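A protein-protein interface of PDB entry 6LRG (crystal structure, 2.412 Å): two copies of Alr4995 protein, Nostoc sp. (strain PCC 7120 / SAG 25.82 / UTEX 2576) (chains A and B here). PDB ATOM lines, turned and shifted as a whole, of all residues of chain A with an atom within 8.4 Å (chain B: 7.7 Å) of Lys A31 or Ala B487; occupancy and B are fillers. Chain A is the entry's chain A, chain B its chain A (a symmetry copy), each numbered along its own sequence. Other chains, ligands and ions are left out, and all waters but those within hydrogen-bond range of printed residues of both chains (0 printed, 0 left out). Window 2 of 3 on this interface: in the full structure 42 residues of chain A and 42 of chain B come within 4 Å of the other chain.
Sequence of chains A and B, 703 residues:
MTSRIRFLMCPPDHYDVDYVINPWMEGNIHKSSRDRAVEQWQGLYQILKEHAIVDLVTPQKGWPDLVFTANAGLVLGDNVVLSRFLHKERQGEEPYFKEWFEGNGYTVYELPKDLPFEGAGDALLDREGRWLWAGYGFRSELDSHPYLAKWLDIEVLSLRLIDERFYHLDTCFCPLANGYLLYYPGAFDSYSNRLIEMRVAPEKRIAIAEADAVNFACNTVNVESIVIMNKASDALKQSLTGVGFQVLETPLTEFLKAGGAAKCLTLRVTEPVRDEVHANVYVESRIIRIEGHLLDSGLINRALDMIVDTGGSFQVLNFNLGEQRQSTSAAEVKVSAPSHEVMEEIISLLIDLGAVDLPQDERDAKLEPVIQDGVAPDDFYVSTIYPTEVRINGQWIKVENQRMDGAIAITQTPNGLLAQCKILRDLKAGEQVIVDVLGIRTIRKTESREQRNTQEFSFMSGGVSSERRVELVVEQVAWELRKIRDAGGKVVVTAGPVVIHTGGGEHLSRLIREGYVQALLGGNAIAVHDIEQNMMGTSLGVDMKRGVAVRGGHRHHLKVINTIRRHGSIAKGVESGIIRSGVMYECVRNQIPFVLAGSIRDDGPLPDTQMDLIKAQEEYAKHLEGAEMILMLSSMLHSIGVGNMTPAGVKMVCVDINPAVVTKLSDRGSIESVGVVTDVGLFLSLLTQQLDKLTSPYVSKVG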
ATOM      1  N   TYR A  15      -4.132  20.535   6.192  1.00  0.00           N
ATOM      2  CA  TYR A  15      -5.141  20.843   5.204  1.00  0.00           C
ATOM      3  C   TYR A  15      -5.804  19.576   4.703  1.00  0.00           C
ATOM      4  O   TYR A  15      -5.134  18.598   4.387  1.00  0.00           O
ATOM      5  CB  TYR A  15      -4.528  21.622   4.032  1.00  0.00           C
ATOM      6  CG  TYR A  15      -5.483  21.792   2.874  1.00  0.00           C
ATOM      7  CD1 TYR A  15      -6.451  22.790   2.879  1.00  0.00           C
ATOM      8  CD2 TYR A  15      -5.431  20.942   1.789  1.00  0.00           C
ATOM      9  CE1 TYR A  15      -7.344  22.925   1.808  1.00  0.00           C
ATOM     10  CE2 TYR A  15      -6.306  21.065   0.733  1.00  0.00           C
ATOM     11  CZ  TYR A  15      -7.254  22.052   0.745  1.00  0.00           C
ATOM     12  OH  TYR A  15      -8.100  22.154  -0.319  1.00  0.00           O
ATOM     13  N   ASP A  16      -7.129  19.601   4.667  1.00  0.00           N
ATOM     14  CA  ASP A  16      -7.916  18.635   3.922  1.00  0.00           C
ATOM     15  C   ASP A  16      -9.286  19.282   3.728  1.00  0.00           C
ATOM     16  O   ASP A  16      -9.524  20.373   4.226  1.00  0.00           O
ATOM     17  CB  ASP A  16      -8.018  17.290   4.653  1.00  0.00           C
ATOM     18  CG  ASP A  16      -8.180  16.087   3.690  1.00  0.00           C
ATOM     19  OD1 ASP A  16      -8.722  16.250   2.568  1.00  0.00           O
ATOM     20  OD2 ASP A  16      -7.765  14.963   4.058  1.00  0.00           O
ATOM     21  N   VAL A  17     -10.176  18.628   2.995  1.00  0.00           N
ATOM     22  CA  VAL A  17     -11.575  19.027   2.978  1.00  0.00           C
ATOM     23  C   VAL A  17     -12.289  18.160   4.019  1.00  0.00           C
ATOM     24  O   VAL A  17     -12.500  16.963   3.791  1.00  0.00           O
ATOM     25  CB  VAL A  17     -12.228  18.851   1.567  1.00  0.00           C
ATOM     26  CG1 VAL A  17     -13.670  19.273   1.593  1.00  0.00           C
ATOM     27  CG2 VAL A  17     -11.484  19.639   0.520  1.00  0.00           C
ATOM     28  N   ASP A  18     -12.644  18.755   5.155  1.00  0.00           N
ATOM     29  CA  ASP A  18     -13.262  18.027   6.273  1.00  0.00           C
ATOM     30  C   ASP A  18     -14.737  18.295   6.448  1.00  0.00           C
ATOM     31  O   ASP A  18     -15.362  17.698   7.313  1.00  0.00           O
ATOM     32  CB  ASP A  18     -12.569  18.368   7.599  1.00  0.00           C
ATOM     33  CG  ASP A  18     -11.111  17.957   7.613  1.00  0.00           C
ATOM     34  OD1 ASP A  18     -10.774  16.944   6.951  1.00  0.00           O
ATOM     35  OD2 ASP A  18     -10.296  18.648   8.267  1.00  0.00           O
ATOM     36  N   TRP A  24     -18.126  23.893  -3.899  1.00  0.00           N
ATOM     37  CA  TRP A  24     -16.918  23.220  -4.369  1.00  0.00           C
ATOM     38  C   TRP A  24     -16.545  22.058  -3.463  1.00  0.00           C
ATOM     39  O   TRP A  24     -16.044  21.060  -3.935  1.00  0.00           O
ATOM     40  CB  TRP A  24     -15.747  24.209  -4.459  1.00  0.00           C
ATOM     41  CG  TRP A  24     -16.009  25.316  -5.407  1.00  0.00           C
ATOM     42  CD1 TRP A  24     -16.647  26.486  -5.136  1.00  0.00           C
ATOM     43  CD2 TRP A  24     -15.678  25.349  -6.803  1.00  0.00           C
ATOM     44  NE1 TRP A  24     -16.737  27.252  -6.270  1.00  0.00           N
ATOM     45  CE2 TRP A  24     -16.142  26.583  -7.309  1.00  0.00           C
ATOM     46  CE3 TRP A  24     -15.027  24.457  -7.670  1.00  0.00           C
ATOM     47  CZ2 TRP A  24     -15.977  26.957  -8.648  1.00  0.00           C
ATOM     48  CZ3 TRP A  24     -14.861  24.821  -8.999  1.00  0.00           C
ATOM     49  CH2 TRP A  24     -15.332  26.068  -9.477  1.00  0.00           C
ATOM     50  N   MET A  25     -16.776  22.192  -2.165  1.00  0.00           N
ATOM     51  CA  MET A  25     -16.379  21.147  -1.215  1.00  0.00           C
ATOM     52  C   MET A  25     -17.291  19.930  -1.317  1.00  0.00           C
ATOM     53  O   MET A  25     -16.884  18.843  -0.928  1.00  0.00           O
ATOM     54  CB  MET A  25     -16.397  21.660   0.232  1.00  0.00           C
ATOM     55  CG  MET A  25     -15.712  22.969   0.460  1.00  0.00           C
ATOM     56  SD  MET A  25     -15.648  23.481   2.198  1.00  0.00           S
ATOM     57  CE  MET A  25     -14.170  22.631   2.714  1.00  0.00           C
ATOM     58  N   GLU A  26     -18.509  20.117  -1.835  1.00  0.00           N
ATOM     59  CA  GLU A  26     -19.478  19.021  -1.984  1.00  0.00           C
ATOM     60  C   GLU A  26     -18.885  17.838  -2.714  1.00  0.00           C
ATOM     61  O   GLU A  26     -18.351  17.983  -3.819  1.00  0.00           O
ATOM     62  CB  GLU A  26     -20.730  19.472  -2.740  1.00  0.00           C
ATOM     63  CG  GLU A  26     -21.930  19.864  -1.876  1.00  0.00           C
ATOM     64  CD  GLU A  26     -22.555  18.694  -1.150  1.00  0.00           C
ATOM     65  OE1 GLU A  26     -22.287  17.544  -1.548  1.00  0.00           O
ATOM     66  OE2 GLU A  26     -23.318  18.917  -0.181  1.00  0.00           O
ATOM     67  N   GLY A  27     -18.972  16.668  -2.106  1.00  0.00           N
ATOM     68  CA  GLY A  27     -18.390  15.476  -2.700  1.00  0.00           C
ATOM     69  C   GLY A  27     -16.875  15.356  -2.583  1.00  0.00           C
ATOM     70  O   GLY A  27     -16.297  14.428  -3.133  1.00  0.00           O
ATOM     71  N   ASN A  28     -16.221  16.261  -1.865  1.00  0.00           N
ATOM     72  CA  ASN A  28     -14.754  16.242  -1.823  1.00  0.00           C
ATOM     73  C   ASN A  28     -14.167  15.967  -0.445  1.00  0.00           C
ATOM     74  O   ASN A  28     -12.958  16.068  -0.264  1.00  0.00           O
ATOM     75  CB  ASN A  28     -14.166  17.563  -2.339  1.00  0.00           C
ATOM     76  CG  ASN A  28     -14.097  17.627  -3.844  1.00  0.00           C
ATOM     77  OD1 ASN A  28     -14.079  16.601  -4.529  1.00  0.00           O
ATOM     78  ND2 ASN A  28     -14.071  18.842  -4.377  1.00  0.00           N
ATOM     79  N   ILE A  29     -15.004  15.608   0.515  1.00  0.00           N
ATOM     80  CA  ILE A  29     -14.526  15.335   1.862  1.00  0.00           C
ATOM     81  C   ILE A  29     -13.441  14.254   1.844  1.00  0.00           C
ATOM     82  O   ILE A  29     -13.615  13.195   1.264  1.00  0.00           O
ATOM     83  CB  ILE A  29     -15.688  14.939   2.793  1.00  0.00           C
ATOM     84  CG1 ILE A  29     -16.475  16.199   3.156  1.00  0.00           C
ATOM     85  CG2 ILE A  29     -15.179  14.292   4.077  1.00  0.00           C
ATOM     86  CD1 ILE A  29     -17.829  15.937   3.699  1.00  0.00           C
ATOM     87  N   HIS A  30     -12.293  14.596   2.427  1.00  0.00           N
ATOM     88  CA  HIS A  30     -11.095  13.759   2.437  1.00  0.00           C
ATOM     89  C   HIS A  30     -10.642  13.285   1.065  1.00  0.00           C
ATOM     90  O   HIS A  30     -10.101  12.198   0.950  1.00  0.00           O
ATOM     91  CB  HIS A  30     -11.315  12.549   3.335  1.00  0.00           C
ATOM     92  CG  HIS A  30     -11.658  12.905   4.743  1.00  0.00           C
ATOM     93  ND1 HIS A  30     -12.651  12.263   5.452  1.00  0.00           N
ATOM     94  CD2 HIS A  30     -11.157  13.855   5.570  1.00  0.00           C
ATOM     95  CE1 HIS A  30     -12.743  12.795   6.660  1.00  0.00           C
ATOM     96  NE2 HIS A  30     -11.846  13.762   6.757  1.00  0.00           N
ATOM     97  N   LYS A  31     -10.834  14.092   0.030  1.00  0.00           N
ATOM     98  CA  LYS A  31     -10.378  13.692  -1.303  1.00  0.00           C
ATOM     99  C   LYS A  31      -9.166  14.505  -1.726  1.00  0.00           C
ATOM    100  O   LYS A  31      -8.756  14.496  -2.897  1.00  0.00           O
ATOM    101  CB  LYS A  31     -11.508  13.818  -2.332  1.00  0.00           C
ATOM    102  CG  LYS A  31     -12.552  12.697  -2.187  1.00  0.00           C
ATOM    103  CD  LYS A  31     -13.491  12.596  -3.389  1.00  0.00           C
ATOM    104  CE  LYS A  31     -14.254  11.272  -3.364  1.00  0.00           C
ATOM    105  NZ  LYS A  31     -15.080  11.053  -4.612  1.00  0.00           N
ATOM    106  N   SER A  32      -8.565  15.176  -0.751  1.00  0.00           N
ATOM    107  CA  SER A  32      -7.360  15.927  -1.012  1.00  0.00           C
ATOM    108  C   SER A  32      -6.109  15.078  -0.829  1.00  0.00           C
ATOM    109  O   SER A  32      -5.954  14.388   0.177  1.00  0.00           O
ATOM    110  CB  SER A  32      -7.278  17.143  -0.098  1.00  0.00           C
ATOM    111  OG  SER A  32      -5.994  17.721  -0.223  1.00  0.00           O
ATOM    112  N   SER A  33      -5.218  15.128  -1.810  1.00  0.00           N
ATOM    113  CA  SER A  33      -3.921  14.476  -1.691  1.00  0.00           C
ATOM    114  C   SER A  33      -2.965  15.434  -0.994  1.00  0.00           C
ATOM    115  O   SER A  33      -2.635  16.478  -1.545  1.00  0.00           O
ATOM    116  CB  SER A  33      -3.392  14.084  -3.065  1.00  0.00           C
ATOM    117  OG  SER A  33      -1.977  14.041  -3.045  1.00  0.00           O
ATOM    118  N   ARG A  34      -2.533  15.126   0.224  1.00  0.00           N
ATOM    119  CA  ARG A  34      -1.778  16.135   0.949  1.00  0.00           C
ATOM    120  C   ARG A  34      -0.394  16.335   0.324  1.00  0.00           C
ATOM    121  O   ARG A  34       0.196  17.388   0.487  1.00  0.00           O
ATOM    122  CB  ARG A  34      -1.661  15.805   2.441  1.00  0.00           C
ATOM    123  CG  ARG A  34      -1.410  17.085   3.277  1.00  0.00           C
ATOM    124  CD  ARG A  34      -1.325  16.834   4.769  1.00  0.00           C
ATOM    125  NE  ARG A  34      -2.583  17.139   5.447  1.00  0.00           N
ATOM    126  CZ  ARG A  34      -2.929  16.648   6.637  1.00  0.00           C
ATOM    127  NH1 ARG A  34      -2.102  15.829   7.284  1.00  0.00           N
ATOM    128  NH2 ARG A  34      -4.103  16.971   7.177  1.00  0.00           N
ATOM    129  N   ARG A  36       0.169  16.337  -3.176  1.00  0.00           N
ATOM    130  CA  ARG A  36      -0.002  17.298  -4.255  1.00  0.00           C
ATOM    131  C   ARG A  36      -0.341  18.672  -3.669  1.00  0.00           C
ATOM    132  O   ARG A  36       0.118  19.699  -4.168  1.00  0.00           O
ATOM    133  CB  ARG A  36      -1.073  16.845  -5.244  1.00  0.00           C
ATOM    134  CG  ARG A  36      -0.604  16.964  -6.698  1.00  0.00           C
ATOM    135  CD  ARG A  36      -1.734  17.049  -7.716  1.00  0.00           C
ATOM    136  NE  ARG A  36      -2.718  15.986  -7.546  1.00  0.00           N
ATOM    137  CZ  ARG A  36      -2.594  14.764  -8.046  1.00  0.00           C
ATOM    138  NH1 ARG A  36      -3.548  13.861  -7.837  1.00  0.00           N
ATOM    139  NH2 ARG A  36      -1.516  14.446  -8.756  1.00  0.00           N
ATOM    140  N   THR A 253      -5.300  22.775  -8.085  1.00  0.00           N
ATOM    141  CA  THR A 253      -6.508  21.963  -8.088  1.00  0.00           C
ATOM    142  C   THR A 253      -6.839  21.347  -6.742  1.00  0.00           C
ATOM    143  O   THR A 253      -8.005  21.216  -6.409  1.00  0.00           O
ATOM    144  CB  THR A 253      -6.407  20.830  -9.126  1.00  0.00           C
ATOM    145  OG1 THR A 253      -5.153  20.163  -8.974  1.00  0.00           O
ATOM    146  CG2 THR A 253      -6.495  21.377 -10.522  1.00  0.00           C
ATOM    147  N   GLU A 254      -5.839  20.963  -5.958  1.00  0.00           N
ATOM    148  CA  GLU A 254      -6.120  20.444  -4.617  1.00  0.00           C
ATOM    149  C   GLU A 254      -6.797  21.498  -3.734  1.00  0.00           C
ATOM    150  O   GLU A 254      -7.467  21.178  -2.743  1.00  0.00           O
ATOM    151  CB  GLU A 254      -4.831  19.953  -3.950  1.00  0.00           C
ATOM    152  CG  GLU A 254      -4.138  18.796  -4.705  1.00  0.00           C
ATOM    153  CD  GLU A 254      -5.088  17.643  -5.052  1.00  0.00           C
ATOM    154  OE1 GLU A 254      -5.831  17.176  -4.154  1.00  0.00           O
ATOM    155  OE2 GLU A 254      -5.086  17.202  -6.227  1.00  0.00           O
ATOM    156  N   LYS A 257     -10.665  22.026  -4.887  1.00  0.00           N
ATOM    157  CA  LYS A 257     -11.584  21.075  -4.256  1.00  0.00           C
ATOM    158  C   LYS A 257     -12.277  21.660  -3.035  1.00  0.00           C
ATOM    159  O   LYS A 257     -13.390  21.239  -2.700  1.00  0.00           O
ATOM    160  CB  LYS A 257     -10.848  19.794  -3.843  1.00  0.00           C
ATOM    161  CG  LYS A 257     -10.312  18.971  -5.015  1.00  0.00           C
ATOM    162  CD  LYS A 257      -9.488  17.814  -4.480  1.00  0.00           C
ATOM    163  CE  LYS A 257      -8.769  17.067  -5.598  1.00  0.00           C
ATOM    164  NZ  LYS A 257      -7.901  15.979  -5.036  1.00  0.00           N
ATOM    165  N   LEU B 481     -21.570  17.644 -13.220  1.00  0.00           N
ATOM    166  CA  LEU B 481     -21.129  16.380 -13.799  1.00  0.00           C
ATOM    167  C   LEU B 481     -19.608  16.318 -13.985  1.00  0.00           C
ATOM    168  O   LEU B 481     -18.979  15.314 -13.657  1.00  0.00           O
ATOM    169  CB  LEU B 481     -21.821  16.144 -15.142  1.00  0.00           C
ATOM    170  CG  LEU B 481     -23.272  15.695 -15.082  1.00  0.00           C
ATOM    171  CD1 LEU B 481     -23.824  15.498 -16.503  1.00  0.00           C
ATOM    172  CD2 LEU B 481     -23.388  14.412 -14.257  1.00  0.00           C
ATOM    173  N   ARG B 482     -19.016  17.388 -14.508  1.00  0.00           N
ATOM    174  CA  ARG B 482     -17.559  17.422 -14.730  1.00  0.00           C
ATOM    175  C   ARG B 482     -16.813  17.252 -13.427  1.00  0.00           C
ATOM    176  O   ARG B 482     -15.786  16.572 -13.363  1.00  0.00           O
ATOM    177  CB  ARG B 482     -17.129  18.734 -15.391  1.00  0.00           C
ATOM    178  CG  ARG B 482     -15.638  18.795 -15.720  1.00  0.00           C
ATOM    179  CD  ARG B 482     -15.234  20.113 -16.386  1.00  0.00           C
ATOM    180  NE  ARG B 482     -13.786  20.212 -16.539  1.00  0.00           N
ATOM    181  CZ  ARG B 482     -13.083  19.612 -17.502  1.00  0.00           C
ATOM    182  NH1 ARG B 482     -13.696  18.870 -18.422  1.00  0.00           N
ATOM    183  NH2 ARG B 482     -11.759  19.754 -17.542  1.00  0.00           N
ATOM    184  N   LYS B 483     -17.356  17.874 -12.390  1.00  0.00           N
ATOM    185  CA  LYS B 483     -16.758  17.893 -11.073  1.00  0.00           C
ATOM    186  C   LYS B 483     -16.807  16.521 -10.398  1.00  0.00           C
ATOM    187  O   LYS B 483     -15.839  16.078  -9.784  1.00  0.00           O
ATOM    188  CB  LYS B 483     -17.488  18.934 -10.215  1.00  0.00           C
ATOM    189  CG  LYS B 483     -16.952  19.097  -8.808  1.00  0.00           C
ATOM    190  CD  LYS B 483     -17.823  20.073  -8.019  1.00  0.00           C
ATOM    191  CE  LYS B 483     -17.376  20.154  -6.593  1.00  0.00           C
ATOM    192  NZ  LYS B 483     -18.304  19.403  -5.700  1.00  0.00           N
ATOM    193  N   ILE B 484     -17.954  15.859 -10.491  1.00  0.00           N
ATOM    194  CA  ILE B 484     -18.089  14.526  -9.929  1.00  0.00           C
ATOM    195  C   ILE B 484     -17.178  13.555 -10.665  1.00  0.00           C
ATOM    196  O   ILE B 484     -16.505  12.757 -10.026  1.00  0.00           O
ATOM    197  CB  ILE B 484     -19.537  14.019  -9.987  1.00  0.00           C
ATOM    198  CG1 ILE B 484     -20.439  14.914  -9.142  1.00  0.00           C
ATOM    199  CG2 ILE B 484     -19.620  12.613  -9.447  1.00  0.00           C
ATOM    200  CD1 ILE B 484     -21.903  14.639  -9.346  1.00  0.00           C
ATOM    201  N   ARG B 485     -17.138  13.624 -11.993  1.00  0.00           N
ATOM    202  CA  ARG B 485     -16.273  12.717 -12.747  1.00  0.00           C
ATOM    203  C   ARG B 485     -14.816  12.881 -12.306  1.00  0.00           C
ATOM    204  O   ARG B 485     -14.124  11.905 -12.000  1.00  0.00           O
ATOM    205  CB  ARG B 485     -16.391  12.948 -14.266  1.00  0.00           C
ATOM    206  CG  ARG B 485     -15.660  11.889 -15.094  1.00  0.00           C
ATOM    207  CD  ARG B 485     -15.587  12.211 -16.582  1.00  0.00           C
ATOM    208  NE  ARG B 485     -14.865  13.451 -16.860  1.00  0.00           N
ATOM    209  CZ  ARG B 485     -14.542  13.876 -18.083  1.00  0.00           C
ATOM    210  NH1 ARG B 485     -14.871  13.159 -19.152  1.00  0.00           N
ATOM    211  NH2 ARG B 485     -13.901  15.023 -18.241  1.00  0.00           N
ATOM    212  N   ASP B 486     -14.355  14.123 -12.254  1.00  0.00           N
ATOM    213  CA  ASP B 486     -12.970  14.389 -11.893  1.00  0.00           C
ATOM    214  C   ASP B 486     -12.649  13.902 -10.488  1.00  0.00           C
ATOM    215  O   ASP B 486     -11.522  13.494 -10.231  1.00  0.00           O
ATOM    216  CB  ASP B 486     -12.657  15.877 -12.008  1.00  0.00           C
ATOM    217  CG  ASP B 486     -12.751  16.395 -13.450  1.00  0.00           C
ATOM    218  OD1 ASP B 486     -13.181  15.630 -14.370  1.00  0.00           O
ATOM    219  OD2 ASP B 486     -12.403  17.589 -13.658  1.00  0.00           O
ATOM    220  N   ALA B 487     -13.625  13.937  -9.579  1.00  0.00           N
ATOM    221  CA  ALA B 487     -13.395  13.477  -8.201  1.00  0.00           C
ATOM    222  C   ALA B 487     -13.560  11.966  -8.014  1.00  0.00           C
ATOM    223  O   ALA B 487     -13.278  11.441  -6.938  1.00  0.00           O
ATOM    224  CB  ALA B 487     -14.324  14.204  -7.241  1.00  0.00           C
ATOM    225  N   GLY B 488     -14.046  11.265  -9.037  1.00  0.00           N
ATOM    226  CA  GLY B 488     -14.260   9.830  -8.926  1.00  0.00           C
ATOM    227  C   GLY B 488     -15.479   9.455  -8.106  1.00  0.00           C
ATOM    228  O   GLY B 488     -15.513   8.398  -7.484  1.00  0.00           O
ATOM    229  N   GLY B 489     -16.479  10.332  -8.097  1.00  0.00           N
ATOM    230  CA  GLY B 489     -17.736  10.065  -7.433  1.00  0.00           C
ATOM    231  C   GLY B 489     -18.680   9.323  -8.359  1.00  0.00           C
ATOM    232  O   GLY B 489     -18.284   8.891  -9.436  1.00  0.00           O
ATOM    233  N   LYS B 490     -19.935   9.203  -7.944  1.00  0.00           N
ATOM    234  CA  LYS B 490     -20.894   8.338  -8.605  1.00  0.00           C
ATOM    235  C   LYS B 490     -22.139   9.100  -9.086  1.00  0.00           C
ATOM    236  O   LYS B 490     -22.848   9.703  -8.288  1.00  0.00           O
ATOM    237  CB  LYS B 490     -21.301   7.225  -7.646  1.00  0.00           C
ATOM    238  CG  LYS B 490     -22.247   6.198  -8.242  1.00  0.00           C
ATOM    239  CD  LYS B 490     -22.649   5.174  -7.210  1.00  0.00           C
ATOM    240  CE  LYS B 490     -23.040   3.892  -7.877  1.00  0.00           C
ATOM    241  NZ  LYS B 490     -23.321   2.837  -6.880  1.00  0.00           N
ATOM    242  N   GLU B 628     -24.015  10.476  -5.726  1.00  0.00           N
ATOM    243  CA  GLU B 628     -23.965  11.886  -5.386  1.00  0.00           C
ATOM    244  C   GLU B 628     -24.954  12.657  -6.233  1.00  0.00           C
ATOM    245  O   GLU B 628     -25.341  13.775  -5.890  1.00  0.00           O
ATOM    246  CB  GLU B 628     -22.559  12.434  -5.587  1.00  0.00           C
ATOM    247  CG  GLU B 628     -21.571  12.003  -4.514  1.00  0.00           C
ATOM    248  CD  GLU B 628     -20.149  11.937  -5.026  1.00  0.00           C
ATOM    249  OE1 GLU B 628     -19.982  11.905  -6.260  1.00  0.00           O
ATOM    250  OE2 GLU B 628     -19.196  11.923  -4.211  1.00  0.00           O
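The backbone carbonyl oxygen (O) of Trp A24 sits close to the side-chain amino group (NZ) of Lys B483 (3.3 Å).
NZ of Lys A31 is in hydrogen-bond range of O of Ala B487.
O of Glu A26 sits close to NZ of Lys B483 (2.4 Å).
The side-chain amide nitrogen (ND2) of Asn A28 sits at hydrogen-bond distance from the backbone carbonyl oxygen (O) of Trp A24, 3.0 Å away.
The side-chain amide nitrogen of Asn A28 lies within hydrogen-bond range of the backbone carbonyl oxygen of Lys A257.
O of Lys A31 sits at hydrogen-bond distance from NZ of Lys A257, 2.7 Å away.
The backbone NH of Gly B489 lies within hydrogen-bond range of the backbone carbonyl oxygen of Ile B484 (3.1 Å).
O of Lys B490 lies within hydrogen-bond range of N of Glu B628 (2.9 Å).
Among the printed residues, merely in contact across the chains: Asn A28 with Ala B487 (3.6 Å), Lys A31 with Gly B489 (3.8 Å), Lys A31 with Gly B488 (3.9 Å) and Gly A27 with Glu B628 (3.9 Å).
Lys A31 touches three residues of chain B.
Of chain A, only Asn A28 (3.6 Å) and Lys A31 (3.0 Å) come within 4 Å of Ala B487.
Gly B488 touches one residue of chain A.
Of the printed residues of chain B, Trp A24 touches Lys B483.
Printed residues of chain A within 4 Å of Glu B628: Gly A27.
Printed residues of chain B within 4 Å of Glu A26: Lys B483.
Printed residues of chain B within 4 Å of Asn A28: Ala B487 (3.6 Å).
Of the printed residues of chain A, Lys B483 touches Trp A24 and Glu A26.
Printed residues of chain B that touch a printed residue of chain A: Lys B483, Ala B487, Gly B488, Gly B489 and Glu B628.
Among the printed residues, 7 pairs touch across the chains.
No position is printed for both chains.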
